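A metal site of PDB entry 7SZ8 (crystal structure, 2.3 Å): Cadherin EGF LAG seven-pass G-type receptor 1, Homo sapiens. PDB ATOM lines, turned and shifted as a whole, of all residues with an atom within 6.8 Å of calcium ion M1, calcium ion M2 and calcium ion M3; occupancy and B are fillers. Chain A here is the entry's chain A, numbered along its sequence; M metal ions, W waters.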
ATOM      1  N   GLU A 245      14.985  29.066  -7.687  1.00  0.00           N
ATOM      2  CA  GLU A 245      16.077  28.865  -8.680  1.00  0.00           C
ATOM      3  C   GLU A 245      15.535  29.040 -10.123  1.00  0.00           C
ATOM      4  O   GLU A 245      16.368  29.171 -11.051  1.00  0.00           O
ATOM      5  CB  GLU A 245      16.741  27.525  -8.404  1.00  0.00           C
ATOM      6  CG  GLU A 245      15.907  26.351  -8.860  1.00  0.00           C
ATOM      7  CD  GLU A 245      16.651  25.034  -8.796  1.00  0.00           C
ATOM      8  OE1 GLU A 245      16.083  24.066  -8.246  1.00  0.00           O
ATOM      9  OE2 GLU A 245      17.792  24.979  -9.305  1.00  0.00           O
ATOM     10  N   LEU A 295      20.244  31.105 -11.502  1.00  0.00           N
ATOM     11  CA  LEU A 295      20.553  30.540 -10.158  1.00  0.00           C
ATOM     12  C   LEU A 295      20.331  29.035 -10.214  1.00  0.00           C
ATOM     13  O   LEU A 295      19.413  28.637 -10.954  1.00  0.00           O
ATOM     14  CB  LEU A 295      19.625  31.190  -9.136  1.00  0.00           C
ATOM     15  CG  LEU A 295      19.845  32.688  -8.977  1.00  0.00           C
ATOM     16  CD1 LEU A 295      18.707  33.354  -8.192  1.00  0.00           C
ATOM     17  CD2 LEU A 295      21.200  32.942  -8.335  1.00  0.00           C
ATOM     18  N   ASP A 296      21.130  28.247  -9.495  1.00  0.00           N
ATOM     19  CA  ASP A 296      20.953  26.768  -9.446  1.00  0.00           C
ATOM     20  C   ASP A 296      21.037  26.284  -8.003  1.00  0.00           C
ATOM     21  O   ASP A 296      22.154  26.214  -7.441  1.00  0.00           O
ATOM     22  CB  ASP A 296      21.931  26.032 -10.358  1.00  0.00           C
ATOM     23  CG  ASP A 296      21.773  24.508 -10.473  1.00  0.00           C
ATOM     24  OD1 ASP A 296      20.939  23.907  -9.756  1.00  0.00           O
ATOM     25  OD2 ASP A 296      22.537  23.914 -11.254  1.00  0.00           O
ATOM     26  N   TYR A 297      19.889  25.900  -7.453  1.00  0.00           N
ATOM     27  CA  TYR A 297      19.795  25.267  -6.120  1.00  0.00           C
ATOM     28  C   TYR A 297      20.793  24.112  -5.988  1.00  0.00           C
ATOM     29  O   TYR A 297      21.354  23.945  -4.882  1.00  0.00           O
ATOM     30  CB  TYR A 297      18.373  24.784  -5.819  1.00  0.00           C
ATOM     31  CG  TYR A 297      18.202  24.261  -4.426  1.00  0.00           C
ATOM     32  CD1 TYR A 297      18.471  22.933  -4.152  1.00  0.00           C
ATOM     33  CD2 TYR A 297      17.807  25.079  -3.382  1.00  0.00           C
ATOM     34  CE1 TYR A 297      18.337  22.428  -2.874  1.00  0.00           C
ATOM     35  CE2 TYR A 297      17.648  24.586  -2.097  1.00  0.00           C
ATOM     36  CZ  TYR A 297      17.915  23.249  -1.846  1.00  0.00           C
ATOM     37  OH  TYR A 297      17.783  22.707  -0.588  1.00  0.00           O
ATOM     38  N   GLU A 298      20.989  23.306  -7.049  1.00  0.00           N
ATOM     39  CA  GLU A 298      21.860  22.089  -6.989  1.00  0.00           C
ATOM     40  C   GLU A 298      23.346  22.484  -6.912  1.00  0.00           C
ATOM     41  O   GLU A 298      24.170  21.593  -6.691  1.00  0.00           O
ATOM     42  CB  GLU A 298      21.582  21.156  -8.173  1.00  0.00           C
ATOM     43  CG  GLU A 298      20.271  20.368  -8.043  1.00  0.00           C
ATOM     44  CD  GLU A 298      18.978  21.178  -7.923  1.00  0.00           C
ATOM     45  OE1 GLU A 298      18.631  21.931  -8.858  1.00  0.00           O
ATOM     46  OE2 GLU A 298      18.323  21.044  -6.918  1.00  0.00           O
ATOM     47  N   ASN A 299      23.657  23.771  -7.059  1.00  0.00           N
ATOM     48  CA  ASN A 299      25.037  24.326  -7.077  1.00  0.00           C
ATOM     49  C   ASN A 299      25.344  25.188  -5.827  1.00  0.00           C
ATOM     50  O   ASN A 299      26.433  24.980  -5.250  1.00  0.00           O
ATOM     51  CB  ASN A 299      25.282  25.115  -8.355  1.00  0.00           C
ATOM     52  CG  ASN A 299      26.636  25.768  -8.339  1.00  0.00           C
ATOM     53  OD1 ASN A 299      26.730  26.984  -8.350  1.00  0.00           O
ATOM     54  ND2 ASN A 299      27.678  24.951  -8.254  1.00  0.00           N
ATOM     55  N   LEU A 328      15.275  28.704  -3.346  1.00  0.00           N
ATOM     56  CA  LEU A 328      14.240  27.646  -3.232  1.00  0.00           C
ATOM     57  C   LEU A 328      14.371  26.695  -4.417  1.00  0.00           C
ATOM     58  O   LEU A 328      14.451  27.166  -5.586  1.00  0.00           O
ATOM     59  CB  LEU A 328      12.846  28.255  -3.171  1.00  0.00           C
ATOM     60  CG  LEU A 328      12.571  29.189  -1.991  1.00  0.00           C
ATOM     61  CD1 LEU A 328      11.102  29.532  -1.949  1.00  0.00           C
ATOM     62  CD2 LEU A 328      13.015  28.610  -0.660  1.00  0.00           C
ATOM     63  N   ASP A 329      14.436  25.403  -4.124  1.00  0.00           N
ATOM     64  CA  ASP A 329      14.555  24.321  -5.129  1.00  0.00           C
ATOM     65  C   ASP A 329      13.296  24.289  -6.014  1.00  0.00           C
ATOM     66  O   ASP A 329      12.212  24.486  -5.512  1.00  0.00           O
ATOM     67  CB  ASP A 329      14.854  22.982  -4.440  1.00  0.00           C
ATOM     68  CG  ASP A 329      14.931  21.793  -5.375  1.00  0.00           C
ATOM     69  OD1 ASP A 329      15.600  21.896  -6.434  1.00  0.00           O
ATOM     70  OD2 ASP A 329      14.311  20.763  -5.020  1.00  0.00           O
ATOM     71  N   ALA A 330      13.492  24.052  -7.301  1.00  0.00           N
ATOM     72  CA  ALA A 330      12.460  23.920  -8.344  1.00  0.00           C
ATOM     73  C   ALA A 330      12.606  22.511  -8.956  1.00  0.00           C
ATOM     74  O   ALA A 330      13.722  21.975  -8.950  1.00  0.00           O
ATOM     75  CB  ALA A 330      12.705  25.028  -9.347  1.00  0.00           C
ATOM     76  N   ASN A 331      11.522  21.925  -9.479  1.00  0.00           N
ATOM     77  CA  ASN A 331      11.600  20.560 -10.063  1.00  0.00           C
ATOM     78  C   ASN A 331      12.223  20.670 -11.460  1.00  0.00           C
ATOM     79  O   ASN A 331      11.524  20.494 -12.461  1.00  0.00           O
ATOM     80  CB  ASN A 331      10.253  19.836 -10.074  1.00  0.00           C
ATOM     81  CG  ASN A 331      10.408  18.335 -10.269  1.00  0.00           C
ATOM     82  OD1 ASN A 331      11.435  17.741  -9.918  1.00  0.00           O
ATOM     83  ND2 ASN A 331       9.392  17.724 -10.857  1.00  0.00           N
ATOM     84  N   ASP A 332      13.517  20.948 -11.522  1.00  0.00           N
ATOM     85  CA  ASP A 332      14.228  21.090 -12.814  1.00  0.00           C
ATOM     86  C   ASP A 332      15.175  19.901 -12.990  1.00  0.00           C
ATOM     87  O   ASP A 332      16.102  20.009 -13.780  1.00  0.00           O
ATOM     88  CB  ASP A 332      14.894  22.478 -12.916  1.00  0.00           C
ATOM     89  CG  ASP A 332      15.968  22.785 -11.879  1.00  0.00           C
ATOM     90  OD1 ASP A 332      16.231  21.914 -10.962  1.00  0.00           O
ATOM     91  OD2 ASP A 332      16.531  23.904 -11.979  1.00  0.00           O
ATOM     92  N   ASN A 333      14.929  18.771 -12.317  1.00  0.00           N
ATOM     93  CA  ASN A 333      15.701  17.526 -12.612  1.00  0.00           C
ATOM     94  C   ASN A 333      14.735  16.354 -12.717  1.00  0.00           C
ATOM     95  O   ASN A 333      13.879  16.198 -11.804  1.00  0.00           O
ATOM     96  CB  ASN A 333      16.802  17.251 -11.578  1.00  0.00           C
ATOM     97  CG  ASN A 333      17.968  18.193 -11.719  1.00  0.00           C
ATOM     98  OD1 ASN A 333      18.918  17.874 -12.436  1.00  0.00           O
ATOM     99  ND2 ASN A 333      17.916  19.357 -11.097  1.00  0.00           N
ATOM    100  N   ALA A 334      14.915  15.554 -13.762  1.00  0.00           N
ATOM    101  CA  ALA A 334      14.139  14.338 -14.093  1.00  0.00           C
ATOM    102  C   ALA A 334      14.810  13.163 -13.407  1.00  0.00           C
ATOM    103  O   ALA A 334      16.021  13.071 -13.419  1.00  0.00           O
ATOM    104  CB  ALA A 334      14.062  14.120 -15.588  1.00  0.00           C
ATOM    105  N   PRO A 335      14.057  12.205 -12.816  1.00  0.00           N
ATOM    106  CA  PRO A 335      14.684  10.983 -12.324  1.00  0.00           C
ATOM    107  C   PRO A 335      15.530  10.306 -13.403  1.00  0.00           C
ATOM    108  O   PRO A 335      15.317  10.557 -14.592  1.00  0.00           O
ATOM    109  CB  PRO A 335      13.493  10.151 -11.873  1.00  0.00           C
ATOM    110  CG  PRO A 335      12.469  11.203 -11.480  1.00  0.00           C
ATOM    111  CD  PRO A 335      12.610  12.251 -12.562  1.00  0.00           C
ATOM    112  N   ASP A 363      17.453  11.450  -8.301  1.00  0.00           N
ATOM    113  CA  ASP A 363      16.886  12.764  -8.694  1.00  0.00           C
ATOM    114  C   ASP A 363      17.678  13.800  -7.903  1.00  0.00           C
ATOM    115  O   ASP A 363      17.682  13.729  -6.642  1.00  0.00           O
ATOM    116  CB  ASP A 363      15.359  12.819  -8.490  1.00  0.00           C
ATOM    117  CG  ASP A 363      14.712  14.121  -8.925  1.00  0.00           C
ATOM    118  OD1 ASP A 363      15.379  15.182  -8.807  1.00  0.00           O
ATOM    119  OD2 ASP A 363      13.507  14.089  -9.378  1.00  0.00           O
ATOM    120  N   ARG A 364      18.309  14.735  -8.625  1.00  0.00           N
ATOM    121  CA  ARG A 364      19.291  15.684  -8.043  1.00  0.00           C
ATOM    122  C   ARG A 364      18.561  16.743  -7.204  1.00  0.00           C
ATOM    123  O   ARG A 364      19.193  17.331  -6.329  1.00  0.00           O
ATOM    124  CB  ARG A 364      20.178  16.258  -9.152  1.00  0.00           C
ATOM    125  CG  ARG A 364      20.965  15.211  -9.912  1.00  0.00           C
ATOM    126  CD  ARG A 364      21.709  15.904 -11.023  1.00  0.00           C
ATOM    127  NE  ARG A 364      22.672  16.870 -10.485  1.00  0.00           N
ATOM    128  CZ  ARG A 364      22.618  18.202 -10.640  1.00  0.00           C
ATOM    129  NH1 ARG A 364      21.630  18.771 -11.313  1.00  0.00           N
ATOM    130  NH2 ARG A 364      23.573  18.959 -10.122  1.00  0.00           N
ATOM    131  N   ASP A 365      17.254  16.910  -7.407  1.00  0.00           N
ATOM    132  CA  ASP A 365      16.370  17.805  -6.616  1.00  0.00           C
ATOM    133  C   ASP A 365      16.265  17.293  -5.171  1.00  0.00           C
ATOM    134  O   ASP A 365      16.588  16.114  -4.897  1.00  0.00           O
ATOM    135  CB  ASP A 365      14.997  17.938  -7.298  1.00  0.00           C
ATOM    136  CG  ASP A 365      15.061  18.600  -8.680  1.00  0.00           C
ATOM    137  OD1 ASP A 365      15.756  19.632  -8.821  1.00  0.00           O
ATOM    138  OD2 ASP A 365      14.411  18.079  -9.594  1.00  0.00           O
ATOM    139  N   SER A 366      15.804  18.159  -4.263  1.00  0.00           N
ATOM    140  CA  SER A 366      15.545  17.850  -2.823  1.00  0.00           C
ATOM    141  C   SER A 366      14.033  17.910  -2.570  1.00  0.00           C
ATOM    142  O   SER A 366      13.291  18.333  -3.498  1.00  0.00           O
ATOM    143  CB  SER A 366      16.312  18.811  -1.927  1.00  0.00           C
ATOM    144  OG  SER A 366      17.607  19.093  -2.460  1.00  0.00           O
ATOM    145  N   PRO A 368       9.988  16.996  -1.939  1.00  0.00           N
ATOM    146  CA  PRO A 368       9.106  16.371  -2.944  1.00  0.00           C
ATOM    147  C   PRO A 368       9.691  16.297  -4.372  1.00  0.00           C
ATOM    148  O   PRO A 368       9.455  15.301  -5.091  1.00  0.00           O
ATOM    149  CB  PRO A 368       7.856  17.265  -2.917  1.00  0.00           C
ATOM    150  CG  PRO A 368       7.813  17.864  -1.504  1.00  0.00           C
ATOM    151  CD  PRO A 368       9.265  17.964  -1.087  1.00  0.00           C
ATOM    152  N   ASN A 369      10.474  17.300  -4.758  1.00  0.00           N
ATOM    153  CA  ASN A 369      11.077  17.362  -6.108  1.00  0.00           C
ATOM    154  C   ASN A 369      11.994  16.154  -6.310  1.00  0.00           C
ATOM    155  O   ASN A 369      12.136  15.691  -7.475  1.00  0.00           O
ATOM    156  CB  ASN A 369      11.776  18.703  -6.317  1.00  0.00           C
ATOM    157  CG  ASN A 369      10.826  19.879  -6.224  1.00  0.00           C
ATOM    158  OD1 ASN A 369       9.677  19.763  -6.649  1.00  0.00           O
ATOM    159  ND2 ASN A 369      11.275  20.987  -5.674  1.00  0.00           N
ATOM    160  N   GLY A 370      12.630  15.671  -5.237  1.00  0.00           N
ATOM    161  CA  GLY A 370      13.679  14.625  -5.270  1.00  0.00           C
ATOM    162  C   GLY A 370      13.185  13.242  -4.861  1.00  0.00           C
ATOM    163  O   GLY A 370      13.941  12.291  -5.103  1.00  0.00           O
ATOM    164  N   ARG A 371      11.971  13.150  -4.298  1.00  0.00           N
ATOM    165  CA  ARG A 371      11.335  11.926  -3.727  1.00  0.00           C
ATOM    166  C   ARG A 371      10.580  11.118  -4.811  1.00  0.00           C
ATOM    167  O   ARG A 371       9.767  11.690  -5.528  1.00  0.00           O
ATOM    168  CB  ARG A 371      10.360  12.340  -2.632  1.00  0.00           C
ATOM    169  CG  ARG A 371       9.941  11.208  -1.703  1.00  0.00           C
ATOM    170  CD  ARG A 371       9.118  11.755  -0.575  1.00  0.00           C
ATOM    171  NE  ARG A 371       8.120  10.781  -0.136  1.00  0.00           N
ATOM    172  CZ  ARG A 371       7.038  11.057   0.582  1.00  0.00           C
ATOM    173  NH1 ARG A 371       6.778  12.309   0.964  1.00  0.00           N
ATOM    174  NH2 ARG A 371       6.216  10.090   0.939  1.00  0.00           N
ATOM    175  N   LEU A 372      10.782   9.804  -4.845  1.00  0.00           N
ATOM    176  CA  LEU A 372      10.528   8.938  -6.030  1.00  0.00           C
ATOM    177  C   LEU A 372       9.407   7.909  -5.767  1.00  0.00           C
ATOM    178  O   LEU A 372       9.330   7.341  -4.662  1.00  0.00           O
ATOM    179  CB  LEU A 372      11.868   8.293  -6.416  1.00  0.00           C
ATOM    180  CG  LEU A 372      12.901   9.279  -6.963  1.00  0.00           C
ATOM    181  CD1 LEU A 372      14.260   8.651  -7.132  1.00  0.00           C
ATOM    182  CD2 LEU A 372      12.438   9.878  -8.278  1.00  0.00           C
ATOM    183  N   ASP A 417       9.018  11.657  -9.769  1.00  0.00           N
ATOM    184  CA  ASP A 417       9.179  12.521  -8.563  1.00  0.00           C
ATOM    185  C   ASP A 417       7.795  13.042  -8.152  1.00  0.00           C
ATOM    186  O   ASP A 417       6.846  12.902  -8.933  1.00  0.00           O
ATOM    187  CB  ASP A 417      10.204  13.634  -8.795  1.00  0.00           C
ATOM    188  CG  ASP A 417       9.928  14.602  -9.929  1.00  0.00           C
ATOM    189  OD1 ASP A 417       8.714  14.992 -10.151  1.00  0.00           O
ATOM    190  OD2 ASP A 417      10.925  14.983 -10.598  1.00  0.00           O
ATOM    191  N   ARG A 418       7.712  13.655  -6.971  1.00  0.00           N
ATOM    192  CA  ARG A 418       6.480  14.294  -6.428  1.00  0.00           C
ATOM    193  C   ARG A 418       6.569  15.829  -6.554  1.00  0.00           C
ATOM    194  O   ARG A 418       6.149  16.522  -5.635  1.00  0.00           O
ATOM    195  CB  ARG A 418       6.323  13.885  -4.966  1.00  0.00           C
ATOM    196  CG  ARG A 418       6.712  12.436  -4.684  1.00  0.00           C
ATOM    197  CD  ARG A 418       6.094  11.418  -5.617  1.00  0.00           C
ATOM    198  NE  ARG A 418       6.277  10.111  -5.006  1.00  0.00           N
ATOM    199  CZ  ARG A 418       5.454   9.552  -4.092  1.00  0.00           C
ATOM    200  NH1 ARG A 418       4.337  10.164  -3.719  1.00  0.00           N
ATOM    201  NH2 ARG A 418       5.752   8.372  -3.588  1.00  0.00           N
ATOM    202  N   GLY A 419       7.104  16.335  -7.664  1.00  0.00           N
ATOM    203  CA  GLY A 419       7.316  17.779  -7.865  1.00  0.00           C
ATOM    204  C   GLY A 419       6.006  18.465  -8.174  1.00  0.00           C
ATOM    205  O   GLY A 419       5.232  17.922  -8.995  1.00  0.00           O
ATOM    206  N   LEU A 424       8.038  15.255 -12.796  1.00  0.00           N
ATOM    207  CA  LEU A 424       8.912  14.688 -13.877  1.00  0.00           C
ATOM    208  C   LEU A 424       9.074  13.179 -13.687  1.00  0.00           C
ATOM    209  O   LEU A 424       8.908  12.710 -12.548  1.00  0.00           O
ATOM    210  CB  LEU A 424      10.288  15.354 -13.929  1.00  0.00           C
ATOM    211  CG  LEU A 424      10.335  16.777 -14.478  1.00  0.00           C
ATOM    212  CD1 LEU A 424      11.620  17.485 -14.061  1.00  0.00           C
ATOM    213  CD2 LEU A 424      10.182  16.798 -15.999  1.00  0.00           C
HETATM  214 CA    CA M   1      12.978  16.082  -9.717  1.00  0.00          CA
HETATM  215 CA    CA M   2      16.211  21.722  -8.523  1.00  0.00          CA
HETATM  216 CA    CA M   3      18.798  23.506 -10.815  1.00  0.00          CA
HETATM  217  O   HOH W   1      19.296  25.018 -12.064  1.00  0.00           O
HETATM  218  O   HOH W   2      19.416  22.026 -12.093  1.00  0.00           O
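Calcium ion M2 is bound by OD1 of Asp 365, OD1 of Asp 329, OE1 of Glu 245, OD1 of Asp 332, OE1 of Glu 298, O of Ala 330 and OE2 of Glu 298.
Of the 27 residues printed, 4 come within 4 Å of calcium ion M3.
Calcium ion M1 is bound by the side-chain carboxylate (OD2) of Asp 363 (2.1 Å), the side-chain amide oxygen (OD1) of Asn 331 (2.3 Å), the backbone carbonyl oxygen (O) of Asn 333 (2.3 Å), the backbone carbonyl oxygen (O) of Asn 369 (2.4 Å), the side-chain carboxylate (OD2) of Asp 365 (2.5 Å), the side-chain carboxylate (OD2) of Asp 417 (2.5 Å) and the side-chain carboxylate (OD1) of Asp 363 (2.7 Å). Calcium ion M1 has seven donor atoms within binding distance.
Calcium ion M3 is bound by water W1 (2.0 Å), water W2 (2.1 Å), the side-chain carboxylate (OE2) of Glu 245 (2.3 Å), the side-chain carboxylate (OD1) of Asp 296 (2.4 Å), the side-chain carboxylate (OE1) of Glu 298 (2.5 Å) and the side-chain carboxylate (OD2) of Asp 332 (2.6 Å). Calcium ion M3 has six donor atoms within binding distance. Slightly farther from calcium ion M3 lies the side-chain carboxylate (OD1) of Asp 332 (3.0 Å).
N of Tyr 297 lies close to OE2 of Glu 245. The side-chain carboxylate (OD1) of Asp 417 is in hydrogen-bond range of the backbone NH (N) of Leu 424 (2.7 Å). The side-chain carboxylate (OD2) of Asp 329 lies within hydrogen-bond range of the backbone NH (N) of Ser 366, 3.1 Å away. OD1 of Asp 332 sits close to ND2 of Asn 333. OD2 of Asp 329 is in hydrogen-bond range of ND2 of Asn 369 (3.1 Å). The backbone NH of Leu 424 lies close to the side-chain amide nitrogen of Asn 331, 3.4 Å away. The side-chain carboxylate (OD1) of Asp 417 is in hydrogen-bond range of the backbone NH (N) of Gly 419 (3.3 Å). ND2 of Asn 333 lies close to OE1 of Glu 298, at 3.5 Å.
Seven residues have an atom within 4 Å of calcium ion M2: Glu 245, Glu 298, Asp 329, Ala 330, Asp 332, Asn 333 and Asp 365. The nearest printed residue that does not touch calcium ion M2 is Tyr 297 (4.6 Å).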
